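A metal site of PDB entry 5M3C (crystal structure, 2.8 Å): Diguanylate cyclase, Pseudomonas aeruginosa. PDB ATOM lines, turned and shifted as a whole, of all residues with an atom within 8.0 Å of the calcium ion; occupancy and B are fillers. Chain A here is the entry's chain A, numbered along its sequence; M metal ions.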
ATOM      1  N   GLN A 196     -15.302  14.245  -4.795  1.00  0.00           N
ATOM      2  CA  GLN A 196     -15.158  13.795  -3.425  1.00  0.00           C
ATOM      3  C   GLN A 196     -15.088  14.996  -2.483  1.00  0.00           C
ATOM      4  O   GLN A 196     -14.356  15.955  -2.744  1.00  0.00           O
ATOM      5  CB  GLN A 196     -13.891  12.951  -3.289  1.00  0.00           C
ATOM      6  CG  GLN A 196     -13.804  12.196  -1.976  1.00  0.00           C
ATOM      7  CD  GLN A 196     -12.764  11.107  -2.018  1.00  0.00           C
ATOM      8  OE1 GLN A 196     -11.800  11.185  -2.774  1.00  0.00           O
ATOM      9  NE2 GLN A 196     -12.956  10.076  -1.205  1.00  0.00           N
ATOM     10  N   LYS A 198     -14.411  17.345   0.966  1.00  0.00           N
ATOM     11  CA  LYS A 198     -13.366  17.568   1.963  1.00  0.00           C
ATOM     12  C   LYS A 198     -13.999  18.136   3.220  1.00  0.00           C
ATOM     13  O   LYS A 198     -15.003  18.831   3.160  1.00  0.00           O
ATOM     14  CB  LYS A 198     -12.329  18.547   1.429  1.00  0.00           C
ATOM     15  CG  LYS A 198     -11.430  17.953   0.359  1.00  0.00           C
ATOM     16  CD  LYS A 198     -10.733  19.038  -0.441  1.00  0.00           C
ATOM     17  CE  LYS A 198      -9.893  18.433  -1.548  1.00  0.00           C
ATOM     18  NZ  LYS A 198      -9.247  19.476  -2.387  1.00  0.00           N
ATOM     19  N   GLU A 210     -12.745  17.385  -4.537  1.00  0.00           N
ATOM     20  CA  GLU A 210     -11.769  17.021  -5.578  1.00  0.00           C
ATOM     21  C   GLU A 210     -12.432  16.322  -6.752  1.00  0.00           C
ATOM     22  O   GLU A 210     -13.303  15.468  -6.582  1.00  0.00           O
ATOM     23  CB  GLU A 210     -10.667  16.120  -5.025  1.00  0.00           C
ATOM     24  CG  GLU A 210      -9.555  15.862  -6.033  1.00  0.00           C
ATOM     25  CD  GLU A 210      -8.476  14.916  -5.530  1.00  0.00           C
ATOM     26  OE1 GLU A 210      -8.472  14.585  -4.330  1.00  0.00           O
ATOM     27  OE2 GLU A 210      -7.630  14.513  -6.361  1.00  0.00           O
ATOM     28  N   ALA A 211     -11.988  16.688  -7.951  1.00  0.00           N
ATOM     29  CA  ALA A 211     -12.461  16.069  -9.173  1.00  0.00           C
ATOM     30  C   ALA A 211     -11.564  14.880  -9.525  1.00  0.00           C
ATOM     31  O   ALA A 211     -10.341  15.001  -9.524  1.00  0.00           O
ATOM     32  CB  ALA A 211     -12.486  17.069 -10.311  1.00  0.00           C
ATOM     33  N   LEU A 212     -12.188  13.754  -9.836  1.00  0.00           N
ATOM     34  CA  LEU A 212     -11.465  12.553 -10.207  1.00  0.00           C
ATOM     35  C   LEU A 212     -11.971  12.039 -11.546  1.00  0.00           C
ATOM     36  O   LEU A 212     -13.179  12.093 -11.824  1.00  0.00           O
ATOM     37  CB  LEU A 212     -11.650  11.474  -9.135  1.00  0.00           C
ATOM     38  CG  LEU A 212     -11.292  11.920  -7.708  1.00  0.00           C
ATOM     39  CD1 LEU A 212     -12.014  11.063  -6.694  1.00  0.00           C
ATOM     40  CD2 LEU A 212      -9.787  11.891  -7.487  1.00  0.00           C
ATOM     41  N   GLU A 226      -5.983   6.669 -10.795  1.00  0.00           N
ATOM     42  CA  GLU A 226      -4.592   6.437 -10.421  1.00  0.00           C
ATOM     43  C   GLU A 226      -3.857   5.702 -11.542  1.00  0.00           C
ATOM     44  O   GLU A 226      -2.681   5.936 -11.779  1.00  0.00           O
ATOM     45  CB  GLU A 226      -4.497   5.612  -9.141  1.00  0.00           C
ATOM     46  CG  GLU A 226      -5.110   6.270  -7.903  1.00  0.00           C
ATOM     47  CD  GLU A 226      -6.613   6.071  -7.804  1.00  0.00           C
ATOM     48  OE1 GLU A 226      -7.192   5.402  -8.704  1.00  0.00           O
ATOM     49  OE2 GLU A 226      -7.220   6.572  -6.840  1.00  0.00           O
ATOM     50  N   ILE A 229      -4.130   8.219 -15.558  1.00  0.00           N
ATOM     51  CA  ILE A 229      -3.224   9.295 -15.967  1.00  0.00           C
ATOM     52  C   ILE A 229      -1.896   8.772 -16.529  1.00  0.00           C
ATOM     53  O   ILE A 229      -1.502   9.142 -17.645  1.00  0.00           O
ATOM     54  CB  ILE A 229      -2.944  10.277 -14.795  1.00  0.00           C
ATOM     55  CG1 ILE A 229      -4.259  10.782 -14.195  1.00  0.00           C
ATOM     56  CG2 ILE A 229      -2.092  11.442 -15.277  1.00  0.00           C
ATOM     57  CD1 ILE A 229      -4.090  11.580 -12.925  1.00  0.00           C
ATOM     58  N   SER A 267     -10.721  20.954  -6.482  1.00  0.00           N
ATOM     59  CA  SER A 267      -9.350  20.479  -6.642  1.00  0.00           C
ATOM     60  C   SER A 267      -9.207  19.535  -7.829  1.00  0.00           C
ATOM     61  O   SER A 267     -10.128  18.766  -8.139  1.00  0.00           O
ATOM     62  CB  SER A 267      -8.895  19.784  -5.367  1.00  0.00           C
ATOM     63  OG  SER A 267      -7.494  19.635  -5.328  1.00  0.00           O
ATOM     64  N   VAL A 268      -8.046  19.562  -8.482  1.00  0.00           N
ATOM     65  CA  VAL A 268      -7.788  18.714  -9.642  1.00  0.00           C
ATOM     66  C   VAL A 268      -6.314  18.329  -9.745  1.00  0.00           C
ATOM     67  O   VAL A 268      -5.442  19.164  -9.537  1.00  0.00           O
ATOM     68  CB  VAL A 268      -8.188  19.428 -10.951  1.00  0.00           C
ATOM     69  CG1 VAL A 268      -7.658  18.661 -12.158  1.00  0.00           C
ATOM     70  CG2 VAL A 268      -9.693  19.570 -11.041  1.00  0.00           C
ATOM     71  N   ASN A 269      -6.047  17.078 -10.091  1.00  0.00           N
ATOM     72  CA  ASN A 269      -4.672  16.635 -10.340  1.00  0.00           C
ATOM     73  C   ASN A 269      -4.144  17.315 -11.601  1.00  0.00           C
ATOM     74  O   ASN A 269      -4.850  17.405 -12.607  1.00  0.00           O
ATOM     75  CB  ASN A 269      -4.593  15.124 -10.498  1.00  0.00           C
ATOM     76  CG  ASN A 269      -4.799  14.377  -9.187  1.00  0.00           C
ATOM     77  OD1 ASN A 269      -4.653  14.946  -8.108  1.00  0.00           O
ATOM     78  ND2 ASN A 269      -5.131  13.099  -9.288  1.00  0.00           N
ATOM     79  N   LEU A 270      -2.908  17.786 -11.540  1.00  0.00           N
ATOM     80  CA  LEU A 270      -2.258  18.361 -12.706  1.00  0.00           C
ATOM     81  C   LEU A 270      -0.991  17.588 -12.995  1.00  0.00           C
ATOM     82  O   LEU A 270      -0.067  17.568 -12.170  1.00  0.00           O
ATOM     83  CB  LEU A 270      -1.921  19.827 -12.472  1.00  0.00           C
ATOM     84  CG  LEU A 270      -1.587  20.610 -13.736  1.00  0.00           C
ATOM     85  CD1 LEU A 270      -2.859  21.018 -14.455  1.00  0.00           C
ATOM     86  CD2 LEU A 270      -0.738  21.828 -13.409  1.00  0.00           C
ATOM     87  N   GLN A 299      -8.207  24.695  -7.537  1.00  0.00           N
ATOM     88  CA  GLN A 299      -7.003  24.204  -6.871  1.00  0.00           C
ATOM     89  C   GLN A 299      -6.316  23.106  -7.683  1.00  0.00           C
ATOM     90  O   GLN A 299      -6.939  22.087  -7.983  1.00  0.00           O
ATOM     91  CB  GLN A 299      -7.351  23.682  -5.476  1.00  0.00           C
ATOM     92  CG  GLN A 299      -6.213  22.988  -4.753  1.00  0.00           C
ATOM     93  CD  GLN A 299      -6.584  22.545  -3.342  1.00  0.00           C
ATOM     94  OE1 GLN A 299      -7.312  23.242  -2.635  1.00  0.00           O
ATOM     95  NE2 GLN A 299      -6.086  21.381  -2.931  1.00  0.00           N
ATOM     96  N   LEU A 300      -5.054  23.316  -8.020  1.00  0.00           N
ATOM     97  CA  LEU A 300      -4.283  22.353  -8.798  1.00  0.00           C
ATOM     98  C   LEU A 300      -3.357  21.521  -7.897  1.00  0.00           C
ATOM     99  O   LEU A 300      -2.533  22.065  -7.162  1.00  0.00           O
ATOM    100  CB  LEU A 300      -3.460  23.069  -9.862  1.00  0.00           C
ATOM    101  CG  LEU A 300      -4.234  24.031 -10.771  1.00  0.00           C
ATOM    102  CD1 LEU A 300      -3.273  24.768 -11.691  1.00  0.00           C
ATOM    103  CD2 LEU A 300      -5.299  23.296 -11.579  1.00  0.00           C
ATOM    104  N   GLU A 301      -3.522  20.199  -7.969  1.00  0.00           N
ATOM    105  CA  GLU A 301      -2.742  19.265  -7.165  1.00  0.00           C
ATOM    106  C   GLU A 301      -1.592  18.686  -7.985  1.00  0.00           C
ATOM    107  O   GLU A 301      -1.839  17.958  -8.953  1.00  0.00           O
ATOM    108  CB  GLU A 301      -3.615  18.108  -6.678  1.00  0.00           C
ATOM    109  CG  GLU A 301      -4.690  18.485  -5.669  1.00  0.00           C
ATOM    110  CD  GLU A 301      -5.517  17.290  -5.236  1.00  0.00           C
ATOM    111  OE1 GLU A 301      -5.139  16.143  -5.552  1.00  0.00           O
ATOM    112  OE2 GLU A 301      -6.554  17.485  -4.557  1.00  0.00           O
ATOM    113  N   ILE A 302      -0.362  18.983  -7.596  1.00  0.00           N
ATOM    114  CA  ILE A 302       0.812  18.411  -8.249  1.00  0.00           C
ATOM    115  C   ILE A 302       1.462  17.366  -7.348  1.00  0.00           C
ATOM    116  O   ILE A 302       1.786  17.654  -6.196  1.00  0.00           O
ATOM    117  CB  ILE A 302       1.862  19.482  -8.601  1.00  0.00           C
ATOM    118  CG1 ILE A 302       1.304  20.482  -9.602  1.00  0.00           C
ATOM    119  CG2 ILE A 302       3.112  18.827  -9.161  1.00  0.00           C
ATOM    120  CD1 ILE A 302       0.412  21.546  -8.979  1.00  0.00           C
ATOM    121  N   THR A 303       1.641  16.159  -7.868  1.00  0.00           N
ATOM    122  CA  THR A 303       2.187  15.052  -7.075  1.00  0.00           C
ATOM    123  C   THR A 303       3.637  15.312  -6.657  1.00  0.00           C
ATOM    124  O   THR A 303       4.446  15.771  -7.451  1.00  0.00           O
ATOM    125  CB  THR A 303       2.111  13.714  -7.836  1.00  0.00           C
ATOM    126  OG1 THR A 303       2.485  12.647  -6.962  1.00  0.00           O
ATOM    127  CG2 THR A 303       3.017  13.709  -9.059  1.00  0.00           C
ATOM    128  N   ALA A 329      -1.553  22.810  -4.636  1.00  0.00           N
ATOM    129  CA  ALA A 329      -1.410  21.832  -3.570  1.00  0.00           C
ATOM    130  C   ALA A 329      -0.420  20.748  -3.963  1.00  0.00           C
ATOM    131  O   ALA A 329      -0.435  20.260  -5.088  1.00  0.00           O
ATOM    132  CB  ALA A 329      -2.759  21.202  -3.254  1.00  0.00           C
ATOM    133  N   ILE A 330       0.452  20.379  -3.023  1.00  0.00           N
ATOM    134  CA  ILE A 330       1.359  19.260  -3.242  1.00  0.00           C
ATOM    135  C   ILE A 330       0.659  17.964  -2.824  1.00  0.00           C
ATOM    136  O   ILE A 330       0.106  17.870  -1.726  1.00  0.00           O
ATOM    137  CB  ILE A 330       2.714  19.425  -2.530  1.00  0.00           C
ATOM    138  CG1 ILE A 330       3.678  18.315  -2.962  1.00  0.00           C
ATOM    139  CG2 ILE A 330       2.545  19.419  -1.016  1.00  0.00           C
ATOM    140  CD1 ILE A 330       5.133  18.592  -2.659  1.00  0.00           C
ATOM    141  N   ASP A 331       0.692  16.990  -3.720  1.00  0.00           N
ATOM    142  CA  ASP A 331      -0.117  15.786  -3.586  1.00  0.00           C
ATOM    143  C   ASP A 331       0.726  14.583  -3.204  1.00  0.00           C
ATOM    144  O   ASP A 331       1.937  14.537  -3.484  1.00  0.00           O
ATOM    145  CB  ASP A 331      -0.846  15.521  -4.909  1.00  0.00           C
ATOM    146  CG  ASP A 331      -2.037  14.595  -4.764  1.00  0.00           C
ATOM    147  OD1 ASP A 331      -2.327  14.149  -3.632  1.00  0.00           O
ATOM    148  OD2 ASP A 331      -2.691  14.310  -5.788  1.00  0.00           O
ATOM    149  N   ASP A 332       0.095  13.604  -2.565  1.00  0.00           N
ATOM    150  CA  ASP A 332       0.733  12.345  -2.200  1.00  0.00           C
ATOM    151  C   ASP A 332       2.057  12.590  -1.493  1.00  0.00           C
ATOM    152  O   ASP A 332       3.093  12.062  -1.906  1.00  0.00           O
ATOM    153  CB  ASP A 332       0.956  11.484  -3.453  1.00  0.00           C
ATOM    154  CG  ASP A 332      -0.344  11.157  -4.162  1.00  0.00           C
ATOM    155  OD1 ASP A 332      -1.301  10.737  -3.490  1.00  0.00           O
ATOM    156  OD2 ASP A 332      -0.393  11.316  -5.397  1.00  0.00           O
ATOM    157  N   LYS A 352      -0.878  17.535   0.937  1.00  0.00           N
ATOM    158  CA  LYS A 352      -1.744  16.372   1.135  1.00  0.00           C
ATOM    159  C   LYS A 352      -0.960  15.162   1.613  1.00  0.00           C
ATOM    160  O   LYS A 352       0.014  14.744   0.979  1.00  0.00           O
ATOM    161  CB  LYS A 352      -2.490  16.041  -0.165  1.00  0.00           C
ATOM    162  CG  LYS A 352      -3.137  17.239  -0.831  1.00  0.00           C
ATOM    163  CD  LYS A 352      -4.155  16.844  -1.882  1.00  0.00           C
ATOM    164  CE  LYS A 352      -5.504  16.512  -1.265  1.00  0.00           C
ATOM    165  NZ  LYS A 352      -6.534  16.194  -2.280  1.00  0.00           N
ATOM    166  N   GLU A 388      -5.567  12.315   3.223  1.00  0.00           N
ATOM    167  CA  GLU A 388      -6.382  11.624   2.223  1.00  0.00           C
ATOM    168  C   GLU A 388      -6.436  10.113   2.477  1.00  0.00           C
ATOM    169  O   GLU A 388      -5.458   9.513   2.925  1.00  0.00           O
ATOM    170  CB  GLU A 388      -5.904  11.930   0.798  1.00  0.00           C
ATOM    171  CG  GLU A 388      -4.413  11.789   0.575  1.00  0.00           C
ATOM    172  CD  GLU A 388      -4.008  12.078  -0.857  1.00  0.00           C
ATOM    173  OE1 GLU A 388      -4.908  12.277  -1.702  1.00  0.00           O
ATOM    174  OE2 GLU A 388      -2.788  12.112  -1.142  1.00  0.00           O
ATOM    175  N   GLN A 408     -10.088  13.862   3.924  1.00  0.00           N
ATOM    176  CA  GLN A 408     -10.716  13.487   2.675  1.00  0.00           C
ATOM    177  C   GLN A 408     -10.669  11.976   2.567  1.00  0.00           C
ATOM    178  O   GLN A 408      -9.612  11.373   2.736  1.00  0.00           O
ATOM    179  CB  GLN A 408      -9.981  14.126   1.503  1.00  0.00           C
ATOM    180  CG  GLN A 408     -10.481  13.712   0.129  1.00  0.00           C
ATOM    181  CD  GLN A 408      -9.681  14.341  -1.004  1.00  0.00           C
ATOM    182  OE1 GLN A 408      -8.749  15.118  -0.768  1.00  0.00           O
ATOM    183  NE2 GLN A 408     -10.045  14.021  -2.238  1.00  0.00           N
HETATM  184 CA    CA M   1      -5.344  14.128  -5.793  1.00  0.00          CA
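OE2 of Glu 301 is in salt-bridge range of NZ of Lys 198, at 3.99 Å. The side-chain carboxylate (OE2) of Glu 301 is in salt-bridge range of the side-chain amino group (NZ) of Lys 352, 2.6 Å away. The backbone carbonyl oxygen (O) of Glu 301 is in hydrogen-bond range of the backbone NH (N) of Leu 270, 2.8 Å away. OE2 of Glu 301 lies within hydrogen-bond range of OG of Ser 267, 2.5 Å away. O of Gln 196 sits at hydrogen-bond distance from N of Glu 210, at 2.8 Å. OE1 of Glu 210 sits at hydrogen-bond distance from NE2 of Gln 408 (2.7 Å). N of Asp 331 lies within hydrogen-bond range of O of Ile 302, 2.8 Å away. The side-chain carboxylate (OE1) of Glu 210 lies within salt-bridge range of the side-chain amino group (NZ) of Lys 352 (3.2 Å).
Of the 23 residues printed, 4 come within 4 Å of the calcium ion. The nearest printed residue that does not touch the calcium ion is Lys 352 (4.2 Å).
The calcium ion is bound by OE1 of Glu 301. The calcium ion is bound by the side-chain carboxylate (OE2) of Glu 210, at 2.4 Å. The calcium ion is bound by OD1 of Asn 269, 2.6 Å away. OD2 of Asp 331 is bound to the calcium ion (2.7 Å).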
